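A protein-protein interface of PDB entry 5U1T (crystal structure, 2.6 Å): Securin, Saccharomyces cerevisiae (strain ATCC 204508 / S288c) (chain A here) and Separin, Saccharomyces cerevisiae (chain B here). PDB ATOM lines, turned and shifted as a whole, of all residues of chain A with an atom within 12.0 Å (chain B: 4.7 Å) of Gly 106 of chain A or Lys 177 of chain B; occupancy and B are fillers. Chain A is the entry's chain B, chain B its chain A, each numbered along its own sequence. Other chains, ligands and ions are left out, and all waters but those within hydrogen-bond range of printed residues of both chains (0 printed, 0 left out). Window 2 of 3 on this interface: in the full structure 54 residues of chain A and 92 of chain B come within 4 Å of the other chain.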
ATOM      1  N   GLU A 105     -22.735  15.611  -4.958  1.00  0.00           N
ATOM      2  CA  GLU A 105     -22.687  14.444  -4.067  1.00  0.00           C
ATOM      3  C   GLU A 105     -21.318  14.191  -3.402  1.00  0.00           C
ATOM      4  O   GLU A 105     -21.112  13.170  -2.730  1.00  0.00           O
ATOM      5  CB  GLU A 105     -23.100  13.190  -4.831  1.00  0.00           C
ATOM      6  CG  GLU A 105     -24.074  12.297  -4.067  1.00  0.00           C
ATOM      7  CD  GLU A 105     -24.942  11.455  -5.002  1.00  0.00           C
ATOM      8  OE1 GLU A 105     -24.487  10.357  -5.411  1.00  0.00           O
ATOM      9  OE2 GLU A 105     -26.071  11.894  -5.333  1.00  0.00           O
ATOM     10  N   GLY A 106     -20.382  15.113  -3.587  1.00  0.00           N
ATOM     11  CA  GLY A 106     -19.066  14.965  -2.998  1.00  0.00           C
ATOM     12  C   GLY A 106     -18.140  13.997  -3.719  1.00  0.00           C
ATOM     13  O   GLY A 106     -18.362  13.628  -4.873  1.00  0.00           O
ATOM     14  N   LEU A 107     -17.074  13.600  -3.038  1.00  0.00           N
ATOM     15  CA  LEU A 107     -16.168  12.609  -3.588  1.00  0.00           C
ATOM     16  C   LEU A 107     -16.891  11.262  -3.739  1.00  0.00           C
ATOM     17  O   LEU A 107     -17.797  10.937  -2.962  1.00  0.00           O
ATOM     18  CB  LEU A 107     -14.936  12.483  -2.695  1.00  0.00           C
ATOM     19  CG  LEU A 107     -14.414  13.835  -2.200  1.00  0.00           C
ATOM     20  CD1 LEU A 107     -13.329  13.646  -1.143  1.00  0.00           C
ATOM     21  CD2 LEU A 107     -13.902  14.673  -3.365  1.00  0.00           C
ATOM     22  N   ASP A 108     -16.516  10.491  -4.755  1.00  0.00           N
ATOM     23  CA  ASP A 108     -17.132   9.186  -4.945  1.00  0.00           C
ATOM     24  C   ASP A 108     -16.331   8.115  -4.210  1.00  0.00           C
ATOM     25  O   ASP A 108     -15.171   8.345  -3.849  1.00  0.00           O
ATOM     26  CB  ASP A 108     -17.290   8.868  -6.444  1.00  0.00           C
ATOM     27  CG  ASP A 108     -16.001   9.014  -7.244  1.00  0.00           C
ATOM     28  OD1 ASP A 108     -14.944   8.466  -6.838  1.00  0.00           O
ATOM     29  OD2 ASP A 108     -16.083   9.653  -8.328  1.00  0.00           O
ATOM     30  N   PRO A 109     -16.960   6.956  -3.947  1.00  0.00           N
ATOM     31  CA  PRO A 109     -16.356   5.870  -3.161  1.00  0.00           C
ATOM     32  C   PRO A 109     -14.868   5.610  -3.393  1.00  0.00           C
ATOM     33  O   PRO A 109     -14.137   5.392  -2.422  1.00  0.00           O
ATOM     34  CB  PRO A 109     -17.180   4.661  -3.586  1.00  0.00           C
ATOM     35  CG  PRO A 109     -18.556   5.239  -3.771  1.00  0.00           C
ATOM     36  CD  PRO A 109     -18.372   6.663  -4.259  1.00  0.00           C
ATOM     37  N   GLU A 110     -14.409   5.640  -4.636  1.00  0.00           N
ATOM     38  CA  GLU A 110     -12.994   5.376  -4.878  1.00  0.00           C
ATOM     39  C   GLU A 110     -12.150   6.581  -4.502  1.00  0.00           C
ATOM     40  O   GLU A 110     -11.023   6.438  -4.017  1.00  0.00           O
ATOM     41  CB  GLU A 110     -12.747   4.990  -6.342  1.00  0.00           C
ATOM     42  CG  GLU A 110     -13.641   3.848  -6.849  1.00  0.00           C
ATOM     43  CD  GLU A 110     -13.428   2.514  -6.101  1.00  0.00           C
ATOM     44  OE1 GLU A 110     -14.249   1.586  -6.334  1.00  0.00           O
ATOM     45  OE2 GLU A 110     -12.463   2.387  -5.297  1.00  0.00           O
ATOM     46  N   GLU A 111     -12.702   7.769  -4.722  1.00  0.00           N
ATOM     47  CA  GLU A 111     -11.990   8.994  -4.393  1.00  0.00           C
ATOM     48  C   GLU A 111     -11.815   9.063  -2.873  1.00  0.00           C
ATOM     49  O   GLU A 111     -10.778   9.508  -2.394  1.00  0.00           O
ATOM     50  CB  GLU A 111     -12.725  10.234  -4.955  1.00  0.00           C
ATOM     51  CG  GLU A 111     -12.656  10.355  -6.496  1.00  0.00           C
ATOM     52  CD  GLU A 111     -13.239  11.656  -7.069  1.00  0.00           C
ATOM     53  OE1 GLU A 111     -14.415  11.999  -6.787  1.00  0.00           O
ATOM     54  OE2 GLU A 111     -12.492  12.333  -7.820  1.00  0.00           O
ATOM     55  N   LEU A 112     -12.805   8.583  -2.121  1.00  0.00           N
ATOM     56  CA  LEU A 112     -12.720   8.562  -0.662  1.00  0.00           C
ATOM     57  C   LEU A 112     -11.593   7.664  -0.153  1.00  0.00           C
ATOM     58  O   LEU A 112     -10.894   8.017   0.795  1.00  0.00           O
ATOM     59  CB  LEU A 112     -14.051   8.118  -0.057  1.00  0.00           C
ATOM     60  CG  LEU A 112     -15.127   9.204  -0.082  1.00  0.00           C
ATOM     61  CD1 LEU A 112     -16.424   8.705   0.513  1.00  0.00           C
ATOM     62  CD2 LEU A 112     -14.631  10.437   0.640  1.00  0.00           C
ATOM     63  N   GLU A 113     -11.412   6.510  -0.787  1.00  0.00           N
ATOM     64  CA  GLU A 113     -10.369   5.574  -0.374  1.00  0.00           C
ATOM     65  C   GLU A 113      -8.973   6.024  -0.787  1.00  0.00           C
ATOM     66  O   GLU A 113      -8.005   5.746  -0.084  1.00  0.00           O
ATOM     67  CB  GLU A 113     -10.657   4.190  -0.933  1.00  0.00           C
ATOM     68  CG  GLU A 113     -11.910   3.579  -0.342  1.00  0.00           C
ATOM     69  CD  GLU A 113     -12.432   2.404  -1.155  1.00  0.00           C
ATOM     70  OE1 GLU A 113     -11.965   1.265  -0.917  1.00  0.00           O
ATOM     71  OE2 GLU A 113     -13.309   2.617  -2.022  1.00  0.00           O
ATOM     72  N   ASP A 114      -8.866   6.729  -1.909  1.00  0.00           N
ATOM     73  CA  ASP A 114      -7.580   7.288  -2.324  1.00  0.00           C
ATOM     74  C   ASP A 114      -7.043   8.266  -1.287  1.00  0.00           C
ATOM     75  O   ASP A 114      -5.834   8.378  -1.080  1.00  0.00           O
ATOM     76  CB  ASP A 114      -7.683   8.013  -3.672  1.00  0.00           C
ATOM     77  CG  ASP A 114      -6.322   8.554  -4.138  1.00  0.00           C
ATOM     78  OD1 ASP A 114      -5.874   9.603  -3.605  1.00  0.00           O
ATOM     79  OD2 ASP A 114      -5.678   7.913  -5.012  1.00  0.00           O
ATOM     80  N   LEU A 115      -7.974   8.974  -0.665  1.00  0.00           N
ATOM     81  CA  LEU A 115      -7.715  10.067   0.262  1.00  0.00           C
ATOM     82  C   LEU A 115      -7.040   9.608   1.547  1.00  0.00           C
ATOM     83  O   LEU A 115      -6.121  10.261   2.063  1.00  0.00           O
ATOM     84  CB  LEU A 115      -9.056  10.750   0.576  1.00  0.00           C
ATOM     85  CG  LEU A 115      -9.222  11.895   1.564  1.00  0.00           C
ATOM     86  CD1 LEU A 115      -8.606  13.150   1.011  1.00  0.00           C
ATOM     87  CD2 LEU A 115     -10.704  12.099   1.801  1.00  0.00           C
ATOM     88  N   GLN B 138     -17.154  15.722   3.834  1.00  0.00           N
ATOM     89  CA  GLN B 138     -17.909  14.720   3.086  1.00  0.00           C
ATOM     90  C   GLN B 138     -19.160  14.334   3.855  1.00  0.00           C
ATOM     91  O   GLN B 138     -20.257  14.304   3.289  1.00  0.00           O
ATOM     92  CB  GLN B 138     -17.042  13.481   2.806  1.00  0.00           C
ATOM     93  CG  GLN B 138     -17.727  12.317   2.074  1.00  0.00           C
ATOM     94  CD  GLN B 138     -18.173  12.666   0.654  1.00  0.00           C
ATOM     95  OE1 GLN B 138     -17.706  13.640   0.056  1.00  0.00           O
ATOM     96  NE2 GLN B 138     -19.092  11.866   0.113  1.00  0.00           N
ATOM     97  N   LEU B 141     -21.731  17.023   4.045  1.00  0.00           N
ATOM     98  CA  LEU B 141     -22.389  17.027   2.760  1.00  0.00           C
ATOM     99  C   LEU B 141     -23.437  15.922   2.652  1.00  0.00           C
ATOM    100  O   LEU B 141     -24.587  16.200   2.352  1.00  0.00           O
ATOM    101  CB  LEU B 141     -21.358  16.882   1.655  1.00  0.00           C
ATOM    102  CG  LEU B 141     -21.965  17.119   0.288  1.00  0.00           C
ATOM    103  CD1 LEU B 141     -22.572  18.507   0.249  1.00  0.00           C
ATOM    104  CD2 LEU B 141     -20.877  16.957  -0.745  1.00  0.00           C
ATOM    105  N   ALA B 172      -5.538  18.096  -3.311  1.00  0.00           N
ATOM    106  CA  ALA B 172      -6.116  19.213  -4.046  1.00  0.00           C
ATOM    107  C   ALA B 172      -7.462  18.872  -4.658  1.00  0.00           C
ATOM    108  O   ALA B 172      -8.495  19.334  -4.172  1.00  0.00           O
ATOM    109  CB  ALA B 172      -5.155  19.676  -5.128  1.00  0.00           C
ATOM    110  N   HIS B 173      -7.437  18.079  -5.732  1.00  0.00           N
ATOM    111  CA  HIS B 173      -8.645  17.692  -6.457  1.00  0.00           C
ATOM    112  C   HIS B 173      -9.797  17.343  -5.512  1.00  0.00           C
ATOM    113  O   HIS B 173     -10.917  17.780  -5.716  1.00  0.00           O
ATOM    114  CB  HIS B 173      -8.362  16.513  -7.393  1.00  0.00           C
ATOM    115  CG  HIS B 173      -9.528  16.157  -8.254  1.00  0.00           C
ATOM    116  ND1 HIS B 173     -10.024  17.011  -9.220  1.00  0.00           N
ATOM    117  CD2 HIS B 173     -10.339  15.069  -8.262  1.00  0.00           C
ATOM    118  CE1 HIS B 173     -11.077  16.455  -9.798  1.00  0.00           C
ATOM    119  NE2 HIS B 173     -11.292  15.280  -9.234  1.00  0.00           N
ATOM    120  N   ALA B 174      -9.508  16.597  -4.449  1.00  0.00           N
ATOM    121  CA  ALA B 174     -10.531  16.243  -3.462  1.00  0.00           C
ATOM    122  C   ALA B 174     -11.117  17.475  -2.779  1.00  0.00           C
ATOM    123  O   ALA B 174     -12.325  17.727  -2.878  1.00  0.00           O
ATOM    124  CB  ALA B 174      -9.969  15.303  -2.439  1.00  0.00           C
ATOM    125  N   LEU B 175     -10.263  18.241  -2.102  1.00  0.00           N
ATOM    126  CA  LEU B 175     -10.690  19.443  -1.383  1.00  0.00           C
ATOM    127  C   LEU B 175     -11.445  20.449  -2.273  1.00  0.00           C
ATOM    128  O   LEU B 175     -12.467  21.009  -1.867  1.00  0.00           O
ATOM    129  CB  LEU B 175      -9.482  20.135  -0.740  1.00  0.00           C
ATOM    130  CG  LEU B 175      -9.767  21.472  -0.049  1.00  0.00           C
ATOM    131  CD1 LEU B 175     -10.677  21.286   1.141  1.00  0.00           C
ATOM    132  CD2 LEU B 175      -8.497  22.179   0.366  1.00  0.00           C
ATOM    133  N   THR B 176     -10.942  20.679  -3.481  1.00  0.00           N
ATOM    134  CA  THR B 176     -11.517  21.708  -4.330  1.00  0.00           C
ATOM    135  C   THR B 176     -12.817  21.189  -4.934  1.00  0.00           C
ATOM    136  O   THR B 176     -13.753  21.953  -5.181  1.00  0.00           O
ATOM    137  CB  THR B 176     -10.539  22.144  -5.440  1.00  0.00           C
ATOM    138  OG1 THR B 176     -10.509  21.152  -6.474  1.00  0.00           O
ATOM    139  CG2 THR B 176      -9.120  22.334  -4.885  1.00  0.00           C
ATOM    140  N   LYS B 177     -12.880  19.878  -5.145  1.00  0.00           N
ATOM    141  CA  LYS B 177     -14.122  19.249  -5.577  1.00  0.00           C
ATOM    142  C   LYS B 177     -15.165  19.356  -4.469  1.00  0.00           C
ATOM    143  O   LYS B 177     -16.348  19.577  -4.732  1.00  0.00           O
ATOM    144  CB  LYS B 177     -13.892  17.788  -5.949  1.00  0.00           C
ATOM    145  CG  LYS B 177     -15.052  17.143  -6.628  1.00  0.00           C
ATOM    146  CD  LYS B 177     -14.825  15.671  -6.851  1.00  0.00           C
ATOM    147  CE  LYS B 177     -15.996  15.086  -7.631  1.00  0.00           C
ATOM    148  NZ  LYS B 177     -15.991  13.602  -7.633  1.00  0.00           N
ATOM    149  N   ILE B 178     -14.716  19.190  -3.225  1.00  0.00           N
ATOM    150  CA  ILE B 178     -15.583  19.317  -2.059  1.00  0.00           C
ATOM    151  C   ILE B 178     -16.194  20.719  -2.013  1.00  0.00           C
ATOM    152  O   ILE B 178     -17.365  20.878  -1.682  1.00  0.00           O
ATOM    153  CB  ILE B 178     -14.804  18.992  -0.752  1.00  0.00           C
ATOM    154  CG1 ILE B 178     -14.858  17.490  -0.472  1.00  0.00           C
ATOM    155  CG2 ILE B 178     -15.370  19.731   0.431  1.00  0.00           C
ATOM    156  CD1 ILE B 178     -16.271  16.948  -0.311  1.00  0.00           C
ATOM    157  N   VAL B 179     -15.404  21.720  -2.394  1.00  0.00           N
ATOM    158  CA  VAL B 179     -15.846  23.112  -2.428  1.00  0.00           C
ATOM    159  C   VAL B 179     -16.949  23.378  -3.466  1.00  0.00           C
ATOM    160  O   VAL B 179     -17.932  24.070  -3.187  1.00  0.00           O
ATOM    161  CB  VAL B 179     -14.658  24.051  -2.711  1.00  0.00           C
ATOM    162  CG1 VAL B 179     -15.123  25.493  -2.871  1.00  0.00           C
ATOM    163  CG2 VAL B 179     -13.644  23.944  -1.599  1.00  0.00           C
ATOM    164  N   LEU B 180     -16.764  22.821  -4.644  1.00  0.00           N
ATOM    165  CA  LEU B 180     -17.708  22.981  -5.705  1.00  0.00           C
ATOM    166  C   LEU B 180     -18.998  22.348  -5.311  1.00  0.00           C
ATOM    167  O   LEU B 180     -20.058  22.887  -5.558  1.00  0.00           O
ATOM    168  CB  LEU B 180     -17.205  22.295  -6.952  1.00  0.00           C
ATOM    169  CG  LEU B 180     -18.230  22.320  -8.071  1.00  0.00           C
ATOM    170  CD1 LEU B 180     -18.245  23.713  -8.657  1.00  0.00           C
ATOM    171  CD2 LEU B 180     -17.899  21.289  -9.130  1.00  0.00           C
ATOM    172  N   SER B 181     -18.919  21.202  -4.662  1.00  0.00           N
ATOM    173  CA  SER B 181     -20.126  20.525  -4.261  1.00  0.00           C
ATOM    174  C   SER B 181     -20.853  21.275  -3.153  1.00  0.00           C
ATOM    175  O   SER B 181     -22.056  21.218  -3.062  1.00  0.00           O
ATOM    176  CB  SER B 181     -19.856  19.072  -3.934  1.00  0.00           C
ATOM    177  OG  SER B 181     -19.702  18.913  -2.560  1.00  0.00           O
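OE1 of Gln 138 of chain B sits at hydrogen-bond distance from N of Leu 107 of chain A, at 3.2 Å. OE2 of Glu 111 of chain A is in hydrogen-bond range of NE2 of His 173 of chain B (3.5 Å). The side-chain amino group (NZ) of Lys 177 of chain B lies within salt-bridge range of the side-chain carboxylate (OE1) of Glu 111 of chain A (2.4 Å).
The side-chain carboxylate (OD1) of Asp 108 of chain A lies close to the backbone NH (N) of Glu 111 of chain A (3.2 Å). The backbone carbonyl oxygen of Ile 178 of chain B lies within hydrogen-bond range of the side-chain hydroxyl of Ser 181 of chain B (3.2 Å). O of His 173 of chain B sits at hydrogen-bond distance from OG1 of Thr 176 of chain B (3.5 Å).
Gln 138 of chain B touches Glu 105 of chain A. C of Glu 105 of chain A touches CD2 of Leu 141 of chain B (3.9 Å). Gln 138 of chain B touches Gly 106 of chain A. Gly 106 of chain A touches Leu 141 of chain B. Gly 106 of chain A touches Lys 177 of chain B (O to NZ, 3.6 Å). Ser 181 of chain B touches Gly 106 of chain A (OG to N, 3.99 Å). Leu 107 of chain A touches Ala 174 of chain B. Lys 177 of chain B touches Leu 107 of chain A. CD2 of Leu 112 of chain A touches CG of Gln 138 of chain B (3.9 Å).
Of the printed residues of chain B, Gly 106 of chain A touches Gln 138, Leu 141, Lys 177 and Ser 181. Of the printed residues of chain A, Lys 177 of chain B touches Gly 106 (3.6 Å), Leu 107 (3.7 Å) and Glu 111 (2.4 Å). Gln 138 of chain B touches just these residues of chain A: Glu 105 (3.7 Å), Gly 106 (3.6 Å), Leu 107 (3.2 Å) and Leu 112 (3.9 Å). Ala 172 of chain B touches none of the printed residues of chain A. His 173 of chain B touches just one residue of chain A: Glu 111. Printed residues of chain A within 4 Å of Ala 174 of chain B: Leu 107 (3.5 Å). No residue of chain A comes within 4 Å of Val 179 of chain B. Of the printed residues of chain B, Leu 112 of chain A touches Gln 138. Printed residues of chain B within 4 Å of Glu 111 of chain A: His 173 (3.5 Å) and Lys 177 (2.4 Å). Of the printed residues of chain A, Ser 181 of chain B touches Gly 106 (3.99 Å). Of the printed residues of chain B, Leu 107 of chain A touches Gln 138 (3.2 Å), Ala 174 (3.5 Å) and Lys 177 (3.7 Å). Of the printed residues of chain B, Glu 105 of chain A touches Gln 138 and Leu 141. Leu 115 of chain A touches none of the printed residues of chain B. Pro 109 of chain A touches none of the printed residues of chain B. The nearest printed residue of chain B that does not touch Gly 106 of chain A is Ile 178 of chain B (4.4 Å). The nearest printed residue of chain A that does not touch Lys 177 of chain B is Asp 108 of chain A (4.01 Å). The nearest printed residue of chain B that does not touch Glu 105 of chain A is Ser 181 of chain B (4.6 Å).
Printed residues of chain B that touch a printed residue of chain A: Gln 138, Leu 141, His 173, Ala 174, Lys 177 and Ser 181. Hydrophobic or aromatic side chains of chain B within 4 Å of the printed part of chain A: Leu 141, His 173 and Ala 174. Of the 11 printed residues of chain A, 5 touch a printed residue of chain B. Among the printed residues, 12 pairs touch across the chains. Among the printed residues, Asp or Glu carboxylates within 4 Å of a Lys or Arg side-chain nitrogen of the other chain: Glu 111 of chain A with Lys 177 of chain B (2.4 Å).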
